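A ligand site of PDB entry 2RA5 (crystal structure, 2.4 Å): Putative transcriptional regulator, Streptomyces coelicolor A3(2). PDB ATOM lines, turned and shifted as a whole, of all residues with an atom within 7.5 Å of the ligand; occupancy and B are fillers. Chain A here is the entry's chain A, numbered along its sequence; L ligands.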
ATOM      1  N   ARG A  73      26.269 -12.554 -18.510  1.00  0.00           N
ATOM      2  CA  ARG A  73      27.104 -13.744 -18.593  1.00  0.00           C
ATOM      3  C   ARG A  73      26.550 -14.678 -19.666  1.00  0.00           C
ATOM      4  O   ARG A  73      25.347 -14.920 -19.718  1.00  0.00           O
ATOM      5  CB  ARG A  73      27.111 -14.479 -17.250  1.00  0.00           C
ATOM      6  CG  ARG A  73      27.600 -13.636 -16.087  1.00  0.00           C
ATOM      7  CD  ARG A  73      27.545 -14.445 -14.786  1.00  0.00           C
ATOM      8  NE  ARG A  73      28.069 -13.697 -13.656  1.00  0.00           N
ATOM      9  CZ  ARG A  73      28.319 -14.235 -12.463  1.00  0.00           C
ATOM     10  NH1 ARG A  73      28.087 -15.531 -12.251  1.00  0.00           N
ATOM     11  NH2 ARG A  73      28.803 -13.475 -11.472  1.00  0.00           N
ATOM     12  N   PRO A 105      25.544 -27.441 -14.298  1.00  0.00           N
ATOM     13  CA  PRO A 105      26.298 -28.662 -14.119  1.00  0.00           C
ATOM     14  C   PRO A 105      25.833 -29.432 -12.871  1.00  0.00           C
ATOM     15  O   PRO A 105      24.850 -29.049 -12.224  1.00  0.00           O
ATOM     16  CB  PRO A 105      27.648 -28.061 -13.726  1.00  0.00           C
ATOM     17  CG  PRO A 105      27.190 -26.638 -12.981  1.00  0.00           C
ATOM     18  CD  PRO A 105      25.664 -26.650 -13.086  1.00  0.00           C
ATOM     19  N   ARG A 138      33.731 -27.638  -3.321  1.00  0.00           N
ATOM     20  CA  ARG A 138      32.865 -28.339  -4.260  1.00  0.00           C
ATOM     21  C   ARG A 138      33.590 -28.699  -5.560  1.00  0.00           C
ATOM     22  O   ARG A 138      34.400 -27.929  -6.068  1.00  0.00           O
ATOM     23  CB  ARG A 138      31.625 -27.524  -4.656  1.00  0.00           C
ATOM     24  CG  ARG A 138      30.673 -27.161  -3.569  1.00  0.00           C
ATOM     25  CD  ARG A 138      30.599 -25.642  -3.478  1.00  0.00           C
ATOM     26  NE  ARG A 138      29.450 -25.056  -4.169  1.00  0.00           N
ATOM     27  CZ  ARG A 138      29.389 -23.782  -4.539  1.00  0.00           C
ATOM     28  NH1 ARG A 138      28.315 -23.321  -5.162  1.00  0.00           N
ATOM     29  NH2 ARG A 138      30.426 -22.983  -4.312  1.00  0.00           N
ATOM     30  N   ARG A 140      32.505 -29.318  -9.438  1.00  0.00           N
ATOM     31  CA  ARG A 140      31.415 -29.187 -10.411  1.00  0.00           C
ATOM     32  C   ARG A 140      31.710 -30.072 -11.602  1.00  0.00           C
ATOM     33  O   ARG A 140      32.794 -30.016 -12.176  1.00  0.00           O
ATOM     34  CB  ARG A 140      31.287 -27.755 -10.890  1.00  0.00           C
ATOM     35  CG  ARG A 140      30.685 -26.844  -9.864  1.00  0.00           C
ATOM     36  CD  ARG A 140      29.186 -26.708 -10.007  1.00  0.00           C
ATOM     37  NE  ARG A 140      28.814 -25.323  -9.732  1.00  0.00           N
ATOM     38  CZ  ARG A 140      27.995 -24.939  -8.760  1.00  0.00           C
ATOM     39  NH1 ARG A 140      27.389 -25.838  -7.987  1.00  0.00           N
ATOM     40  NH2 ARG A 140      27.744 -23.643  -8.586  1.00  0.00           N
ATOM     41  N   LEU A 150      35.838 -25.641  -6.646  1.00  0.00           N
ATOM     42  CA  LEU A 150      35.388 -24.413  -5.969  1.00  0.00           C
ATOM     43  C   LEU A 150      35.617 -24.416  -4.457  1.00  0.00           C
ATOM     44  O   LEU A 150      34.919 -25.116  -3.730  1.00  0.00           O
ATOM     45  CB  LEU A 150      33.895 -24.196  -6.226  1.00  0.00           C
ATOM     46  CG  LEU A 150      33.340 -24.317  -7.655  1.00  0.00           C
ATOM     47  CD1 LEU A 150      31.880 -23.895  -7.698  1.00  0.00           C
ATOM     48  CD2 LEU A 150      34.178 -23.500  -8.645  1.00  0.00           C
ATOM     49  N   CYS A 151      36.580 -23.617  -3.976  1.00  0.00           N
ATOM     50  CA  CYS A 151      36.754 -23.400  -2.525  1.00  0.00           C
ATOM     51  C   CYS A 151      36.140 -22.076  -2.087  1.00  0.00           C
ATOM     52  O   CYS A 151      36.502 -21.019  -2.603  1.00  0.00           O
ATOM     53  CB  CYS A 151      38.241 -23.408  -2.119  1.00  0.00           C
ATOM     54  SG  CYS A 151      39.240 -24.761  -2.784  1.00  0.00           S
ATOM     55  N   ASN A 152      35.230 -22.128  -1.117  1.00  0.00           N
ATOM     56  CA  ASN A 152      34.660 -20.893  -0.567  1.00  0.00           C
ATOM     57  C   ASN A 152      34.790 -20.710   0.946  1.00  0.00           C
ATOM     58  O   ASN A 152      34.808 -21.681   1.710  1.00  0.00           O
ATOM     59  CB  ASN A 152      33.198 -20.686  -1.009  1.00  0.00           C
ATOM     60  CG  ASN A 152      33.041 -20.668  -2.524  1.00  0.00           C
ATOM     61  OD1 ASN A 152      33.017 -19.612  -3.156  1.00  0.00           O
ATOM     62  ND2 ASN A 152      32.981 -21.842  -3.124  1.00  0.00           N
ATOM     63  N   LEU A 166      23.759 -27.948  -0.825  1.00  0.00           N
ATOM     64  CA  LEU A 166      24.791 -27.454  -1.718  1.00  0.00           C
ATOM     65  C   LEU A 166      24.901 -28.259  -3.000  1.00  0.00           C
ATOM     66  O   LEU A 166      25.436 -27.773  -3.998  1.00  0.00           O
ATOM     67  CB  LEU A 166      26.123 -27.454  -0.975  1.00  0.00           C
ATOM     68  CG  LEU A 166      26.349 -26.169  -0.179  1.00  0.00           C
ATOM     69  CD1 LEU A 166      27.335 -26.389   0.969  1.00  0.00           C
ATOM     70  CD2 LEU A 166      26.803 -25.034  -1.096  1.00  0.00           C
ATOM     71  N   THR A 169      21.444 -26.657  -5.017  1.00  0.00           N
ATOM     72  CA  THR A 169      21.443 -25.299  -5.569  1.00  0.00           C
ATOM     73  C   THR A 169      22.774 -24.549  -5.413  1.00  0.00           C
ATOM     74  O   THR A 169      23.643 -24.935  -4.622  1.00  0.00           O
ATOM     75  CB  THR A 169      20.295 -24.439  -4.974  1.00  0.00           C
ATOM     76  OG1 THR A 169      20.612 -24.066  -3.625  1.00  0.00           O
ATOM     77  CG2 THR A 169      18.990 -25.230  -4.970  1.00  0.00           C
ATOM     78  N   GLY A 170      22.928 -23.472  -6.182  1.00  0.00           N
ATOM     79  CA  GLY A 170      24.099 -22.616  -6.099  1.00  0.00           C
ATOM     80  C   GLY A 170      24.269 -21.910  -4.757  1.00  0.00           C
ATOM     81  O   GLY A 170      23.321 -21.688  -4.002  1.00  0.00           O
ATOM     82  N   LEU A 171      25.500 -21.523  -4.477  1.00  0.00           N
ATOM     83  CA  LEU A 171      25.829 -20.908  -3.203  1.00  0.00           C
ATOM     84  C   LEU A 171      25.178 -19.535  -3.040  1.00  0.00           C
ATOM     85  O   LEU A 171      24.759 -19.176  -1.940  1.00  0.00           O
ATOM     86  CB  LEU A 171      27.358 -20.803  -3.043  1.00  0.00           C
ATOM     87  CG  LEU A 171      27.902 -20.086  -1.807  1.00  0.00           C
ATOM     88  CD1 LEU A 171      27.408 -20.763  -0.539  1.00  0.00           C
ATOM     89  CD2 LEU A 171      29.429 -20.016  -1.841  1.00  0.00           C
ATOM     90  N   TYR A 172      25.076 -18.782  -4.127  1.00  0.00           N
ATOM     91  CA  TYR A 172      24.422 -17.473  -4.088  1.00  0.00           C
ATOM     92  C   TYR A 172      22.939 -17.566  -3.755  1.00  0.00           C
ATOM     93  O   TYR A 172      22.427 -16.763  -2.974  1.00  0.00           O
ATOM     94  CB  TYR A 172      24.598 -16.729  -5.409  1.00  0.00           C
ATOM     95  CG  TYR A 172      25.886 -15.958  -5.509  1.00  0.00           C
ATOM     96  CD1 TYR A 172      26.984 -16.273  -4.711  1.00  0.00           C
ATOM     97  CD2 TYR A 172      26.001 -14.911  -6.421  1.00  0.00           C
ATOM     98  CE1 TYR A 172      28.163 -15.560  -4.801  1.00  0.00           C
ATOM     99  CE2 TYR A 172      27.168 -14.200  -6.518  1.00  0.00           C
ATOM    100  CZ  TYR A 172      28.247 -14.525  -5.713  1.00  0.00           C
ATOM    101  OH  TYR A 172      29.401 -13.793  -5.853  1.00  0.00           O
ATOM    102  N   ARG A 173      22.257 -18.538  -4.362  1.00  0.00           N
ATOM    103  CA  ARG A 173      20.831 -18.747  -4.137  1.00  0.00           C
ATOM    104  C   ARG A 173      20.588 -19.063  -2.674  1.00  0.00           C
ATOM    105  O   ARG A 173      19.686 -18.504  -2.053  1.00  0.00           O
ATOM    106  CB  ARG A 173      20.279 -19.863  -5.037  1.00  0.00           C
ATOM    107  CG  ARG A 173      18.823 -20.269  -4.753  1.00  0.00           C
ATOM    108  CD  ARG A 173      18.342 -21.367  -5.697  1.00  0.00           C
ATOM    109  NE  ARG A 173      17.231 -22.165  -5.153  1.00  0.00           N
ATOM    110  CZ  ARG A 173      16.040 -22.320  -5.745  1.00  0.00           C
ATOM    111  NH1 ARG A 173      15.107 -23.065  -5.155  1.00  0.00           N
ATOM    112  NH2 ARG A 173      15.769 -21.736  -6.899  1.00  0.00           N
ATOM    113  N   LEU A 174      21.415 -19.956  -2.128  1.00  0.00           N
ATOM    114  CA  LEU A 174      21.305 -20.310  -0.714  1.00  0.00           C
ATOM    115  C   LEU A 174      21.457 -19.095   0.180  1.00  0.00           C
ATOM    116  O   LEU A 174      20.698 -18.905   1.123  1.00  0.00           O
ATOM    117  CB  LEU A 174      22.351 -21.367  -0.332  1.00  0.00           C
ATOM    118  CG  LEU A 174      21.864 -22.809  -0.411  1.00  0.00           C
ATOM    119  CD1 LEU A 174      22.998 -23.783  -0.112  1.00  0.00           C
ATOM    120  CD2 LEU A 174      20.722 -23.001   0.567  1.00  0.00           C
ATOM    121  N   MET A 175      22.459 -18.261  -0.118  1.00  0.00           N
ATOM    122  CA  MET A 175      22.732 -17.097   0.721  1.00  0.00           C
ATOM    123  C   MET A 175      21.588 -16.097   0.684  1.00  0.00           C
ATOM    124  O   MET A 175      21.205 -15.534   1.711  1.00  0.00           O
ATOM    125  CB  MET A 175      24.041 -16.420   0.317  1.00  0.00           C
ATOM    126  CG  MET A 175      25.274 -17.322   0.457  1.00  0.00           C
ATOM    127  SD  MET A 175      26.964 -16.394   0.140  1.00  0.00           S
ATOM    128  CE  MET A 175      26.501 -15.467  -1.508  1.00  0.00           C
ATOM    129  N   ARG A 176      21.057 -15.857  -0.508  1.00  0.00           N
ATOM    130  CA  ARG A 176      19.918 -14.968  -0.651  1.00  0.00           C
ATOM    131  C   ARG A 176      18.751 -15.567   0.121  1.00  0.00           C
ATOM    132  O   ARG A 176      18.017 -14.861   0.803  1.00  0.00           O
ATOM    133  CB  ARG A 176      19.568 -14.765  -2.128  1.00  0.00           C
ATOM    134  CG  ARG A 176      20.313 -13.582  -2.745  1.00  0.00           C
ATOM    135  CD  ARG A 176      19.867 -13.288  -4.183  1.00  0.00           C
ATOM    136  NE  ARG A 176      20.344 -14.300  -5.144  1.00  0.00           N
ATOM    137  CZ  ARG A 176      21.246 -14.070  -6.085  1.00  0.00           C
ATOM    138  NH1 ARG A 176      21.784 -12.856  -6.217  1.00  0.00           N
ATOM    139  NH2 ARG A 176      21.617 -15.045  -6.907  1.00  0.00           N
ATOM    140  N   LEU A 182      23.177  -9.550  -1.725  1.00  0.00           N
ATOM    141  CA  LEU A 182      24.419  -9.554  -2.479  1.00  0.00           C
ATOM    142  C   LEU A 182      24.412  -8.318  -3.364  1.00  0.00           C
ATOM    143  O   LEU A 182      23.558  -8.180  -4.235  1.00  0.00           O
ATOM    144  CB  LEU A 182      24.522 -10.845  -3.291  1.00  0.00           C
ATOM    145  CG  LEU A 182      24.325 -12.075  -2.393  1.00  0.00           C
ATOM    146  CD1 LEU A 182      24.274 -13.371  -3.161  1.00  0.00           C
ATOM    147  CD2 LEU A 182      25.429 -12.143  -1.362  1.00  0.00           C
ATOM    148  N   MET A 213      40.135 -18.212 -10.818  1.00  0.00           N
ATOM    149  CA  MET A 213      39.481 -16.976 -10.456  1.00  0.00           C
ATOM    150  C   MET A 213      39.303 -16.806  -8.930  1.00  0.00           C
ATOM    151  O   MET A 213      39.101 -17.766  -8.171  1.00  0.00           O
ATOM    152  CB  MET A 213      38.185 -16.838 -11.237  1.00  0.00           C
ATOM    153  CG  MET A 213      36.957 -17.257 -10.517  1.00  0.00           C
ATOM    154  SD  MET A 213      35.859 -15.697 -10.184  1.00  0.00           S
ATOM    155  CE  MET A 213      34.168 -16.608  -9.828  1.00  0.00           C
ATOM    156  N   ARG A 215      37.224 -14.318  -6.074  1.00  0.00           N
ATOM    157  CA  ARG A 215      36.114 -13.401  -5.965  1.00  0.00           C
ATOM    158  C   ARG A 215      35.798 -13.071  -4.508  1.00  0.00           C
ATOM    159  O   ARG A 215      35.816 -13.955  -3.656  1.00  0.00           O
ATOM    160  CB  ARG A 215      34.897 -14.026  -6.665  1.00  0.00           C
ATOM    161  CG  ARG A 215      33.575 -13.321  -6.445  1.00  0.00           C
ATOM    162  CD  ARG A 215      32.434 -14.201  -6.902  1.00  0.00           C
ATOM    163  NE  ARG A 215      32.295 -15.450  -6.133  1.00  0.00           N
ATOM    164  CZ  ARG A 215      31.628 -16.520  -6.555  1.00  0.00           C
ATOM    165  NH1 ARG A 215      31.545 -17.612  -5.791  1.00  0.00           N
ATOM    166  NH2 ARG A 215      31.032 -16.519  -7.744  1.00  0.00           N
ATOM    167  N   THR A 217      32.579 -11.341  -2.387  1.00  0.00           N
ATOM    168  CA  THR A 217      31.217 -10.813  -2.511  1.00  0.00           C
ATOM    169  C   THR A 217      30.784 -10.033  -1.271  1.00  0.00           C
ATOM    170  O   THR A 217      30.919 -10.510  -0.144  1.00  0.00           O
ATOM    171  CB  THR A 217      30.222 -11.953  -2.776  1.00  0.00           C
ATOM    172  OG1 THR A 217      30.685 -12.736  -3.875  1.00  0.00           O
ATOM    173  CG2 THR A 217      28.828 -11.400  -3.085  1.00  0.00           C
ATOM    174  N   GLU A 226      31.378 -13.495   1.407  1.00  0.00           N
ATOM    175  CA  GLU A 226      31.856 -14.695   0.759  1.00  0.00           C
ATOM    176  C   GLU A 226      33.170 -14.402   0.031  1.00  0.00           C
ATOM    177  O   GLU A 226      33.332 -13.362  -0.607  1.00  0.00           O
ATOM    178  CB  GLU A 226      30.794 -15.216  -0.227  1.00  0.00           C
ATOM    179  CG  GLU A 226      31.191 -16.484  -0.986  1.00  0.00           C
ATOM    180  CD  GLU A 226      31.993 -16.213  -2.278  1.00  0.00           C
ATOM    181  OE1 GLU A 226      31.841 -15.122  -2.881  1.00  0.00           O
ATOM    182  OE2 GLU A 226      32.767 -17.091  -2.692  1.00  0.00           O
ATOM    183  N   GLY A 228      35.793 -16.589  -2.593  1.00  0.00           N
ATOM    184  CA  GLY A 228      35.951 -17.814  -3.349  1.00  0.00           C
ATOM    185  C   GLY A 228      37.265 -17.847  -4.075  1.00  0.00           C
ATOM    186  O   GLY A 228      37.770 -16.835  -4.568  1.00  0.00           O
ATOM    187  N   HIS A 230      38.845 -20.329  -7.006  1.00  0.00           N
ATOM    188  CA  HIS A 230      38.395 -21.375  -7.905  1.00  0.00           C
ATOM    189  C   HIS A 230      39.399 -21.714  -8.990  1.00  0.00           C
ATOM    190  O   HIS A 230      40.177 -20.871  -9.419  1.00  0.00           O
ATOM    191  CB  HIS A 230      37.092 -20.961  -8.571  1.00  0.00           C
ATOM    192  CG  HIS A 230      36.057 -20.466  -7.615  1.00  0.00           C
ATOM    193  ND1 HIS A 230      35.340 -19.318  -7.821  1.00  0.00           N
ATOM    194  CD2 HIS A 230      35.594 -20.984  -6.441  1.00  0.00           C
ATOM    195  CE1 HIS A 230      34.490 -19.128  -6.833  1.00  0.00           C
ATOM    196  NE2 HIS A 230      34.626 -20.145  -5.986  1.00  0.00           N
ATOM    197  N   TYR A 232      39.511 -23.932 -12.892  1.00  0.00           N
ATOM    198  CA  TYR A 232      38.712 -24.470 -13.979  1.00  0.00           C
ATOM    199  C   TYR A 232      39.585 -25.146 -15.012  1.00  0.00           C
ATOM    200  O   TYR A 232      40.616 -24.585 -15.422  1.00  0.00           O
ATOM    201  CB  TYR A 232      37.939 -23.366 -14.678  1.00  0.00           C
ATOM    202  CG  TYR A 232      37.165 -22.466 -13.750  1.00  0.00           C
ATOM    203  CD1 TYR A 232      37.781 -21.376 -13.138  1.00  0.00           C
ATOM    204  CD2 TYR A 232      35.821 -22.693 -13.491  1.00  0.00           C
ATOM    205  CE1 TYR A 232      37.068 -20.548 -12.296  1.00  0.00           C
ATOM    206  CE2 TYR A 232      35.097 -21.866 -12.647  1.00  0.00           C
ATOM    207  CZ  TYR A 232      35.723 -20.797 -12.044  1.00  0.00           C
ATOM    208  OH  TYR A 232      34.999 -19.969 -11.199  1.00  0.00           O
HETATM  209  O1  LIG L   1      30.122 -20.080  -5.878  1.00  0.00           O
HETATM  210  O2  LIG L   1      30.532 -19.983  -8.061  1.00  0.00           O
HETATM  211  C1  LIG L   1      29.788 -20.296  -7.084  1.00  0.00           C
HETATM  212  C2  LIG L   1      28.464 -20.986  -7.360  1.00  0.00           C
HETATM  213  O3  LIG L   1      27.755 -21.200  -6.138  1.00  0.00           O
HETATM  214  C3  LIG L   1      27.623 -20.236  -8.413  1.00  0.00           C
HETATM  215  O4  LIG L   1      26.668 -21.084  -9.055  1.00  0.00           O
HETATM  216  C4  LIG L   1      26.868 -19.095  -7.793  1.00  0.00           C
HETATM  217  O5  LIG L   1      25.691 -19.270  -7.380  1.00  0.00           O
HETATM  218  O6  LIG L   1      27.504 -18.024  -7.743  1.00  0.00           O
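NE of Arg 215 sits close to OH of Tyr 172, at 3.3 Å.
NH2 of Arg 138 lies close to ND2 of Asn 152 (3.0 Å).
The side-chain hydroxyl (OG1) of Thr 217 is in hydrogen-bond range of the side-chain hydroxyl (OH) of Tyr 172, at 2.6 Å.
The backbone carbonyl oxygen (O) of Arg 215 lies within hydrogen-bond range of the backbone NH (N) of Gly 228 (2.8 Å).
The backbone carbonyl oxygen (O) of Arg 138 sits at hydrogen-bond distance from the backbone NH (N) of Leu 150 (2.8 Å).
NE of Arg 215 is in salt-bridge range of OE1 of Glu 226, 3.3 Å away.
C of Gly 170 touches O3 of the ligand, at 3.8 Å.
Hydrophobic or aromatic side chains within 4 Å of the ligand: Leu 171 and Tyr 172.
Six residues have an atom within 4 Å of the ligand: Arg 138, Arg 140, Gly 170, Leu 171, Tyr 172 and Arg 215.
O1 of the ligand lies within salt-bridge range of NH1 of Arg 215.
An oxygen (O5) of the ligand lies within hydrogen-bond range of the backbone NH (N) of Tyr 172 (3.3 Å).
N of Leu 171 lies within hydrogen-bond range of O3 of the ligand, 2.8 Å away.
O1 of the ligand lies within salt-bridge range of NH2 of Arg 138.
NH2 of Arg 140 sits at hydrogen-bond distance from O4 of the ligand (2.8 Å).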
